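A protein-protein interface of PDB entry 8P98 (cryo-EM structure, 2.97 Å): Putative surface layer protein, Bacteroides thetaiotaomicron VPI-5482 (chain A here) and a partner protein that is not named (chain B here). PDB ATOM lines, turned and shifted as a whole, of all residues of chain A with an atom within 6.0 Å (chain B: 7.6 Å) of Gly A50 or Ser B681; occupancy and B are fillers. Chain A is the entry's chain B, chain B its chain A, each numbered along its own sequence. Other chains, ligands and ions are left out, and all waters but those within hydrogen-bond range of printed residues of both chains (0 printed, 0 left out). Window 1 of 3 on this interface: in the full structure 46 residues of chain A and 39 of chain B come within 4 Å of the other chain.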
ATOM      1  N   ASN A  46      -8.188  -8.010  -5.132  1.00  0.00           N
ATOM      2  CA  ASN A  46      -8.339  -9.409  -5.504  1.00  0.00           C
ATOM      3  C   ASN A  46      -9.816  -9.790  -5.595  1.00  0.00           C
ATOM      4  O   ASN A  46     -10.718  -8.965  -5.427  1.00  0.00           O
ATOM      5  CB  ASN A  46      -7.617 -10.314  -4.512  1.00  0.00           C
ATOM      6  CG  ASN A  46      -6.133 -10.397  -4.779  1.00  0.00           C
ATOM      7  OD1 ASN A  46      -5.315 -10.142  -3.897  1.00  0.00           O
ATOM      8  ND2 ASN A  46      -5.774 -10.745  -6.008  1.00  0.00           N
ATOM      9  N   PHE A  47     -10.056 -11.068  -5.865  1.00  0.00           N
ATOM     10  CA  PHE A  47     -11.384 -11.559  -6.196  1.00  0.00           C
ATOM     11  C   PHE A  47     -11.724 -12.718  -5.264  1.00  0.00           C
ATOM     12  O   PHE A  47     -10.966 -13.688  -5.166  1.00  0.00           O
ATOM     13  CB  PHE A  47     -11.414 -11.948  -7.679  1.00  0.00           C
ATOM     14  CG  PHE A  47     -12.761 -12.351  -8.197  1.00  0.00           C
ATOM     15  CD1 PHE A  47     -13.756 -11.410  -8.368  1.00  0.00           C
ATOM     16  CD2 PHE A  47     -12.993 -13.635  -8.636  1.00  0.00           C
ATOM     17  CE1 PHE A  47     -14.988 -11.764  -8.872  1.00  0.00           C
ATOM     18  CE2 PHE A  47     -14.222 -13.997  -9.144  1.00  0.00           C
ATOM     19  CZ  PHE A  47     -15.220 -13.060  -9.264  1.00  0.00           C
ATOM     20  N   GLN A  48     -12.864 -12.600  -4.572  1.00  0.00           N
ATOM     21  CA  GLN A  48     -13.171 -13.363  -3.352  1.00  0.00           C
ATOM     22  C   GLN A  48     -12.112 -13.165  -2.271  1.00  0.00           C
ATOM     23  O   GLN A  48     -11.651 -14.124  -1.651  1.00  0.00           O
ATOM     24  CB  GLN A  48     -13.381 -14.861  -3.600  1.00  0.00           C
ATOM     25  CG  GLN A  48     -14.631 -15.238  -4.366  1.00  0.00           C
ATOM     26  CD  GLN A  48     -14.431 -15.194  -5.847  1.00  0.00           C
ATOM     27  OE1 GLN A  48     -13.302 -15.221  -6.321  1.00  0.00           O
ATOM     28  NE2 GLN A  48     -15.525 -15.133  -6.596  1.00  0.00           N
ATOM     29  N   TYR A  49     -11.721 -11.915  -2.038  1.00  0.00           N
ATOM     30  CA  TYR A  49     -10.912 -11.602  -0.864  1.00  0.00           C
ATOM     31  C   TYR A  49     -11.301 -10.318  -0.152  1.00  0.00           C
ATOM     32  O   TYR A  49     -10.862 -10.121   0.984  1.00  0.00           O
ATOM     33  CB  TYR A  49      -9.424 -11.545  -1.236  1.00  0.00           C
ATOM     34  CG  TYR A  49      -8.864 -12.889  -1.635  1.00  0.00           C
ATOM     35  CD1 TYR A  49      -8.485 -13.813  -0.671  1.00  0.00           C
ATOM     36  CD2 TYR A  49      -8.741 -13.247  -2.969  1.00  0.00           C
ATOM     37  CE1 TYR A  49      -7.981 -15.045  -1.022  1.00  0.00           C
ATOM     38  CE2 TYR A  49      -8.239 -14.480  -3.332  1.00  0.00           C
ATOM     39  CZ  TYR A  49      -7.862 -15.375  -2.354  1.00  0.00           C
ATOM     40  OH  TYR A  49      -7.360 -16.605  -2.707  1.00  0.00           O
ATOM     41  N   GLY A  50     -12.106  -9.451  -0.755  1.00  0.00           N
ATOM     42  CA  GLY A  50     -12.571  -8.255  -0.084  1.00  0.00           C
ATOM     43  C   GLY A  50     -11.465  -7.294   0.293  1.00  0.00           C
ATOM     44  O   GLY A  50     -11.438  -6.781   1.416  1.00  0.00           O
ATOM     45  N   ASN A  51     -10.543  -7.043  -0.630  1.00  0.00           N
ATOM     46  CA  ASN A  51      -9.422  -6.146  -0.385  1.00  0.00           C
ATOM     47  C   ASN A  51      -9.395  -5.028  -1.415  1.00  0.00           C
ATOM     48  O   ASN A  51      -8.331  -4.555  -1.818  1.00  0.00           O
ATOM     49  CB  ASN A  51      -8.102  -6.914  -0.376  1.00  0.00           C
ATOM     50  CG  ASN A  51      -7.825  -7.613  -1.687  1.00  0.00           C
ATOM     51  OD1 ASN A  51      -8.732  -7.847  -2.480  1.00  0.00           O
ATOM     52  ND2 ASN A  51      -6.569  -7.971  -1.910  1.00  0.00           N
ATOM     53  N   ALA A  52     -10.570  -4.591  -1.857  1.00  0.00           N
ATOM     54  CA  ALA A  52     -10.638  -3.455  -2.759  1.00  0.00           C
ATOM     55  C   ALA A  52     -10.227  -2.183  -2.028  1.00  0.00           C
ATOM     56  O   ALA A  52     -10.420  -2.039  -0.819  1.00  0.00           O
ATOM     57  CB  ALA A  52     -12.044  -3.303  -3.335  1.00  0.00           C
ATOM     58  N   LYS A  76     -14.635  -0.524   4.919  1.00  0.00           N
ATOM     59  CA  LYS A  76     -13.959  -0.922   3.693  1.00  0.00           C
ATOM     60  C   LYS A  76     -14.844  -0.692   2.472  1.00  0.00           C
ATOM     61  O   LYS A  76     -16.072  -0.627   2.559  1.00  0.00           O
ATOM     62  CB  LYS A  76     -13.541  -2.388   3.768  1.00  0.00           C
ATOM     63  CG  LYS A  76     -12.465  -2.664   4.794  1.00  0.00           C
ATOM     64  CD  LYS A  76     -12.050  -4.119   4.770  1.00  0.00           C
ATOM     65  CE  LYS A  76     -10.886  -4.374   5.710  1.00  0.00           C
ATOM     66  NZ  LYS A  76     -11.266  -4.179   7.134  1.00  0.00           N
ATOM     67  N   GLY A  78     -15.149  -2.641  -0.334  1.00  0.00           N
ATOM     68  CA  GLY A  78     -15.830  -3.815  -0.843  1.00  0.00           C
ATOM     69  C   GLY A  78     -14.898  -4.792  -1.526  1.00  0.00           C
ATOM     70  O   GLY A  78     -13.801  -5.059  -1.028  1.00  0.00           O
ATOM     71  N   ASP A  79     -15.323  -5.343  -2.659  1.00  0.00           N
ATOM     72  CA  ASP A  79     -14.491  -6.247  -3.438  1.00  0.00           C
ATOM     73  C   ASP A  79     -14.676  -5.962  -4.919  1.00  0.00           C
ATOM     74  O   ASP A  79     -15.796  -5.721  -5.376  1.00  0.00           O
ATOM     75  CB  ASP A  79     -14.819  -7.713  -3.144  1.00  0.00           C
ATOM     76  CG  ASP A  79     -13.609  -8.611  -3.272  1.00  0.00           C
ATOM     77  OD1 ASP A  79     -12.486  -8.079  -3.374  1.00  0.00           O
ATOM     78  OD2 ASP A  79     -13.776  -9.847  -3.263  1.00  0.00           O
ATOM     79  N   TYR B  89     -10.662 -20.516   8.625  1.00  0.00           N
ATOM     80  CA  TYR B  89     -11.521 -19.414   9.052  1.00  0.00           C
ATOM     81  C   TYR B  89     -12.866 -19.898   9.589  1.00  0.00           C
ATOM     82  O   TYR B  89     -13.932 -19.439   9.193  1.00  0.00           O
ATOM     83  CB  TYR B  89     -11.680 -18.413   7.912  1.00  0.00           C
ATOM     84  CG  TYR B  89     -12.359 -18.908   6.656  1.00  0.00           C
ATOM     85  CD1 TYR B  89     -11.619 -19.485   5.636  1.00  0.00           C
ATOM     86  CD2 TYR B  89     -13.716 -18.713   6.443  1.00  0.00           C
ATOM     87  CE1 TYR B  89     -12.220 -19.916   4.475  1.00  0.00           C
ATOM     88  CE2 TYR B  89     -14.325 -19.138   5.285  1.00  0.00           C
ATOM     89  CZ  TYR B  89     -13.573 -19.737   4.303  1.00  0.00           C
ATOM     90  OH  TYR B  89     -14.179 -20.160   3.142  1.00  0.00           O
ATOM     91  N   ASP B 217     -16.164  -3.719   9.558  1.00  0.00           N
ATOM     92  CA  ASP B 217     -15.799  -3.419   8.183  1.00  0.00           C
ATOM     93  C   ASP B 217     -16.958  -2.876   7.360  1.00  0.00           C
ATOM     94  O   ASP B 217     -16.753  -2.503   6.200  1.00  0.00           O
ATOM     95  CB  ASP B 217     -15.232  -4.668   7.496  1.00  0.00           C
ATOM     96  CG  ASP B 217     -14.058  -5.263   8.245  1.00  0.00           C
ATOM     97  OD1 ASP B 217     -13.380  -4.516   8.981  1.00  0.00           O
ATOM     98  OD2 ASP B 217     -13.807  -6.477   8.097  1.00  0.00           O
ATOM     99  N   ALA B 277     -19.485 -19.366   2.461  1.00  0.00           N
ATOM    100  CA  ALA B 277     -19.907 -18.228   3.263  1.00  0.00           C
ATOM    101  C   ALA B 277     -19.710 -16.918   2.511  1.00  0.00           C
ATOM    102  O   ALA B 277     -18.800 -16.774   1.692  1.00  0.00           O
ATOM    103  CB  ALA B 277     -19.137 -18.189   4.583  1.00  0.00           C
ATOM    104  N   LEU B 278     -20.584 -15.958   2.797  1.00  0.00           N
ATOM    105  CA  LEU B 278     -20.487 -14.637   2.200  1.00  0.00           C
ATOM    106  C   LEU B 278     -19.462 -13.788   2.940  1.00  0.00           C
ATOM    107  O   LEU B 278     -19.184 -13.999   4.123  1.00  0.00           O
ATOM    108  CB  LEU B 278     -21.847 -13.942   2.212  1.00  0.00           C
ATOM    109  CG  LEU B 278     -22.788 -14.324   1.071  1.00  0.00           C
ATOM    110  CD1 LEU B 278     -24.038 -13.464   1.089  1.00  0.00           C
ATOM    111  CD2 LEU B 278     -22.073 -14.198  -0.258  1.00  0.00           C
ATOM    112  N   LEU B 279     -18.900 -12.819   2.225  1.00  0.00           N
ATOM    113  CA  LEU B 279     -17.875 -11.960   2.795  1.00  0.00           C
ATOM    114  C   LEU B 279     -18.470 -11.035   3.850  1.00  0.00           C
ATOM    115  O   LEU B 279     -19.685 -10.832   3.928  1.00  0.00           O
ATOM    116  CB  LEU B 279     -17.201 -11.131   1.705  1.00  0.00           C
ATOM    117  CG  LEU B 279     -16.389 -11.892   0.662  1.00  0.00           C
ATOM    118  CD1 LEU B 279     -15.992 -10.965  -0.466  1.00  0.00           C
ATOM    119  CD2 LEU B 279     -15.163 -12.493   1.305  1.00  0.00           C
ATOM    120  N   THR B 280     -17.587 -10.471   4.673  1.00  0.00           N
ATOM    121  CA  THR B 280     -18.016  -9.494   5.668  1.00  0.00           C
ATOM    122  C   THR B 280     -18.661  -8.288   5.001  1.00  0.00           C
ATOM    123  O   THR B 280     -19.747  -7.850   5.396  1.00  0.00           O
ATOM    124  CB  THR B 280     -16.823  -9.065   6.522  1.00  0.00           C
ATOM    125  OG1 THR B 280     -16.338 -10.186   7.268  1.00  0.00           O
ATOM    126  CG2 THR B 280     -17.215  -7.960   7.471  1.00  0.00           C
ATOM    127  N   THR B 281     -18.012  -7.744   3.979  1.00  0.00           N
ATOM    128  CA  THR B 281     -18.554  -6.610   3.234  1.00  0.00           C
ATOM    129  C   THR B 281     -19.318  -7.064   1.994  1.00  0.00           C
ATOM    130  O   THR B 281     -19.088  -6.594   0.882  1.00  0.00           O
ATOM    131  CB  THR B 281     -17.431  -5.646   2.874  1.00  0.00           C
ATOM    132  OG1 THR B 281     -17.949  -4.590   2.057  1.00  0.00           O
ATOM    133  CG2 THR B 281     -16.300  -6.367   2.147  1.00  0.00           C
ATOM    134  N   ASP B 282     -20.259  -7.984   2.186  1.00  0.00           N
ATOM    135  CA  ASP B 282     -21.114  -8.490   1.114  1.00  0.00           C
ATOM    136  C   ASP B 282     -22.552  -8.175   1.500  1.00  0.00           C
ATOM    137  O   ASP B 282     -23.235  -8.995   2.115  1.00  0.00           O
ATOM    138  CB  ASP B 282     -20.910  -9.987   0.895  1.00  0.00           C
ATOM    139  CG  ASP B 282     -21.584 -10.490  -0.370  1.00  0.00           C
ATOM    140  OD1 ASP B 282     -22.827 -10.428  -0.453  1.00  0.00           O
ATOM    141  OD2 ASP B 282     -20.870 -10.958  -1.282  1.00  0.00           O
ATOM    142  N   TYR B 598       0.671 -15.220   4.599  1.00  0.00           N
ATOM    143  CA  TYR B 598      -0.101 -16.146   5.429  1.00  0.00           C
ATOM    144  C   TYR B 598       0.780 -17.206   6.079  1.00  0.00           C
ATOM    145  O   TYR B 598       0.452 -18.392   6.091  1.00  0.00           O
ATOM    146  CB  TYR B 598      -1.223 -16.799   4.626  1.00  0.00           C
ATOM    147  CG  TYR B 598      -2.463 -15.948   4.524  1.00  0.00           C
ATOM    148  CD1 TYR B 598      -3.364 -15.874   5.576  1.00  0.00           C
ATOM    149  CD2 TYR B 598      -2.733 -15.217   3.379  1.00  0.00           C
ATOM    150  CE1 TYR B 598      -4.496 -15.098   5.488  1.00  0.00           C
ATOM    151  CE2 TYR B 598      -3.862 -14.438   3.283  1.00  0.00           C
ATOM    152  CZ  TYR B 598      -4.741 -14.381   4.340  1.00  0.00           C
ATOM    153  OH  TYR B 598      -5.868 -13.604   4.243  1.00  0.00           O
ATOM    154  N   THR B 638      -6.211  -1.669   5.333  1.00  0.00           N
ATOM    155  CA  THR B 638      -7.258  -2.553   4.847  1.00  0.00           C
ATOM    156  C   THR B 638      -6.786  -3.988   4.660  1.00  0.00           C
ATOM    157  O   THR B 638      -7.547  -4.812   4.144  1.00  0.00           O
ATOM    158  CB  THR B 638      -7.824  -2.023   3.530  1.00  0.00           C
ATOM    159  OG1 THR B 638      -8.968  -2.798   3.157  1.00  0.00           O
ATOM    160  CG2 THR B 638      -6.786  -2.115   2.432  1.00  0.00           C
ATOM    161  N   GLY B 639      -5.555  -4.302   5.050  1.00  0.00           N
ATOM    162  CA  GLY B 639      -5.038  -5.648   4.907  1.00  0.00           C
ATOM    163  C   GLY B 639      -4.284  -6.135   6.125  1.00  0.00           C
ATOM    164  O   GLY B 639      -3.322  -6.898   6.000  1.00  0.00           O
ATOM    165  N   HIS B 640      -4.704  -5.701   7.308  1.00  0.00           N
ATOM    166  CA  HIS B 640      -3.996  -5.989   8.547  1.00  0.00           C
ATOM    167  C   HIS B 640      -4.679  -7.128   9.291  1.00  0.00           C
ATOM    168  O   HIS B 640      -5.904  -7.128   9.443  1.00  0.00           O
ATOM    169  CB  HIS B 640      -3.935  -4.748   9.435  1.00  0.00           C
ATOM    170  CG  HIS B 640      -3.284  -4.987  10.761  1.00  0.00           C
ATOM    171  ND1 HIS B 640      -3.806  -4.509  11.943  1.00  0.00           N
ATOM    172  CD2 HIS B 640      -2.151  -5.648  11.091  1.00  0.00           C
ATOM    173  CE1 HIS B 640      -3.024  -4.869  12.944  1.00  0.00           C
ATOM    174  NE2 HIS B 640      -2.011  -5.560  12.455  1.00  0.00           N
ATOM    175  N   LEU B 641      -3.887  -8.088   9.750  1.00  0.00           N
ATOM    176  CA  LEU B 641      -4.381  -9.200  10.562  1.00  0.00           C
ATOM    177  C   LEU B 641      -3.632  -9.227  11.884  1.00  0.00           C
ATOM    178  O   LEU B 641      -2.425  -9.530  11.902  1.00  0.00           O
ATOM    179  CB  LEU B 641      -4.214 -10.529   9.828  1.00  0.00           C
ATOM    180  CG  LEU B 641      -5.059 -10.732   8.570  1.00  0.00           C
ATOM    181  CD1 LEU B 641      -4.702 -12.038   7.896  1.00  0.00           C
ATOM    182  CD2 LEU B 641      -6.533 -10.696   8.909  1.00  0.00           C
ATOM    183  N   LEU B 677     -10.570 -11.959  14.023  1.00  0.00           N
ATOM    184  CA  LEU B 677     -10.494 -12.111  12.574  1.00  0.00           C
ATOM    185  C   LEU B 677      -9.239 -12.906  12.255  1.00  0.00           C
ATOM    186  O   LEU B 677      -8.134 -12.480  12.607  1.00  0.00           O
ATOM    187  CB  LEU B 677     -10.464 -10.747  11.893  1.00  0.00           C
ATOM    188  CG  LEU B 677     -10.586 -10.717  10.374  1.00  0.00           C
ATOM    189  CD1 LEU B 677     -11.961 -11.182   9.969  1.00  0.00           C
ATOM    190  CD2 LEU B 677     -10.320  -9.320   9.854  1.00  0.00           C
ATOM    191  N   SER B 678      -9.402 -14.061  11.608  1.00  0.00           N
ATOM    192  CA  SER B 678      -8.269 -14.903  11.251  1.00  0.00           C
ATOM    193  C   SER B 678      -8.003 -14.967   9.757  1.00  0.00           C
ATOM    194  O   SER B 678      -6.889 -15.325   9.363  1.00  0.00           O
ATOM    195  CB  SER B 678      -8.475 -16.329  11.779  1.00  0.00           C
ATOM    196  OG  SER B 678      -7.659 -17.248  11.076  1.00  0.00           O
ATOM    197  N   VAL B 679      -8.987 -14.646   8.923  1.00  0.00           N
ATOM    198  CA  VAL B 679      -8.815 -14.555   7.480  1.00  0.00           C
ATOM    199  C   VAL B 679      -9.472 -13.264   7.019  1.00  0.00           C
ATOM    200  O   VAL B 679     -10.521 -12.874   7.541  1.00  0.00           O
ATOM    201  CB  VAL B 679      -9.406 -15.780   6.750  1.00  0.00           C
ATOM    202  CG1 VAL B 679      -9.490 -15.538   5.255  1.00  0.00           C
ATOM    203  CG2 VAL B 679      -8.556 -17.003   7.024  1.00  0.00           C
ATOM    204  N   LEU B 680      -8.843 -12.595   6.055  1.00  0.00           N
ATOM    205  CA  LEU B 680      -9.238 -11.245   5.675  1.00  0.00           C
ATOM    206  C   LEU B 680     -10.689 -11.199   5.212  1.00  0.00           C
ATOM    207  O   LEU B 680     -11.096 -11.967   4.336  1.00  0.00           O
ATOM    208  CB  LEU B 680      -8.312 -10.733   4.574  1.00  0.00           C
ATOM    209  CG  LEU B 680      -8.160  -9.217   4.477  1.00  0.00           C
ATOM    210  CD1 LEU B 680      -7.594  -8.673   5.774  1.00  0.00           C
ATOM    211  CD2 LEU B 680      -7.275  -8.841   3.303  1.00  0.00           C
ATOM    212  N   SER B 681     -11.454 -10.277   5.795  1.00  0.00           N
ATOM    213  CA  SER B 681     -12.843 -10.001   5.420  1.00  0.00           C
ATOM    214  C   SER B 681     -13.702 -11.265   5.420  1.00  0.00           C
ATOM    215  O   SER B 681     -14.457 -11.533   4.484  1.00  0.00           O
ATOM    216  CB  SER B 681     -12.918  -9.293   4.065  1.00  0.00           C
ATOM    217  OG  SER B 681     -12.117  -9.931   3.088  1.00  0.00           O
ATOM    218  N   ARG B 682     -13.581 -12.054   6.488  1.00  0.00           N
ATOM    219  CA  ARG B 682     -14.494 -13.175   6.689  1.00  0.00           C
ATOM    220  C   ARG B 682     -14.991 -13.168   8.129  1.00  0.00           C
ATOM    221  O   ARG B 682     -14.184 -13.216   9.064  1.00  0.00           O
ATOM    222  CB  ARG B 682     -13.823 -14.508   6.355  1.00  0.00           C
ATOM    223  CG  ARG B 682     -13.166 -14.534   4.990  1.00  0.00           C
ATOM    224  CD  ARG B 682     -14.169 -14.804   3.886  1.00  0.00           C
ATOM    225  NE  ARG B 682     -14.307 -16.218   3.567  1.00  0.00           N
ATOM    226  CZ  ARG B 682     -14.602 -16.677   2.359  1.00  0.00           C
ATOM    227  NH1 ARG B 682     -14.779 -15.860   1.335  1.00  0.00           N
ATOM    228  NH2 ARG B 682     -14.722 -17.987   2.173  1.00  0.00           N
ATOM    229  N   PRO B 683     -16.303 -13.131   8.345  1.00  0.00           N
ATOM    230  CA  PRO B 683     -16.831 -12.933   9.698  1.00  0.00           C
ATOM    231  C   PRO B 683     -16.494 -14.089  10.622  1.00  0.00           C
ATOM    232  O   PRO B 683     -16.247 -15.218  10.195  1.00  0.00           O
ATOM    233  CB  PRO B 683     -18.342 -12.832   9.479  1.00  0.00           C
ATOM    234  CG  PRO B 683     -18.582 -13.534   8.195  1.00  0.00           C
ATOM    235  CD  PRO B 683     -17.377 -13.277   7.350  1.00  0.00           C
ATOM    236  N   MET B 684     -16.485 -13.785  11.915  1.00  0.00           N
ATOM    237  CA  MET B 684     -16.185 -14.762  12.944  1.00  0.00           C
ATOM    238  C   MET B 684     -17.281 -14.745  13.998  1.00  0.00           C
ATOM    239  O   MET B 684     -17.891 -13.701  14.246  1.00  0.00           O
ATOM    240  CB  MET B 684     -14.839 -14.461  13.614  1.00  0.00           C
ATOM    241  CG  MET B 684     -13.653 -14.956  12.831  1.00  0.00           C
ATOM    242  SD  MET B 684     -13.620 -16.735  12.629  1.00  0.00           S
ATOM    243  CE  MET B 684     -13.041 -16.809  10.944  1.00  0.00           C
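Gln A48 touches none of the printed residues of chain B.
Of the printed residues of chain B, Tyr A49 touches Leu B680 (3.8 Å) and Ser B681 (2.5 Å).
Of chain B, only Ser B681 comes within 4 Å of Gly A50.
Printed residues of chain B within 4 Å of Lys A76: Asp B217 (2.8 Å) and Thr B638 (3.6 Å).
Of the printed residues of chain A, Thr B638 touches Lys A76.
Ser B678 touches none of the printed residues of chain A.
Ser B681 touches two residues of chain A.
The nearest residue of chain A that does not touch Ser B681 is Asn A51 (5.0 Å).
The backbone carbonyl oxygen of Ser B681 is in hydrogen-bond range of the backbone NH of Thr B280 (3.3 Å).
The side-chain carboxylate (OD2) of Asp A79 lies within hydrogen-bond range of the backbone NH (N) of Gln A48.
The backbone NH (N) of Tyr A49 lies within hydrogen-bond range of the side-chain carboxylate (OD2) of Asp A79 (3.2 Å).
N of Gly A50 sits at hydrogen-bond distance from OD1 of Asp A79 (3.0 Å).
The backbone NH of Ala A52 lies within hydrogen-bond range of the backbone carbonyl oxygen of Gly A78, at 3.4 Å.
Among the printed residues, merely in contact across the chains: Tyr A49 with Leu B680, Gly A50 with Ser B681, Lys A76 with Thr B638, Gly A78 with Thr B281 and Asp A79 with Leu B279.
The side-chain carboxylate (OD1) of Asp B217 is in salt-bridge range of the side-chain amino group (NZ) of Lys A76 (2.8 Å).
The side-chain hydroxyl of Ser B681 is in hydrogen-bond range of the backbone carbonyl oxygen of Tyr A49 (2.5 Å).
Hydrophobic or aromatic side chains of chain B that line the printed part of chain A: Leu B279.
Of the 10 printed residues of chain A, 5 touch a printed residue of chain B.
Printed residues of chain A that touch a printed residue of chain B: Tyr A49, Gly A50, Lys A76, Gly A78 and Asp A79.
Along chain A the printed residues that touch a printed residue of chain B span positions 49 to 79.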
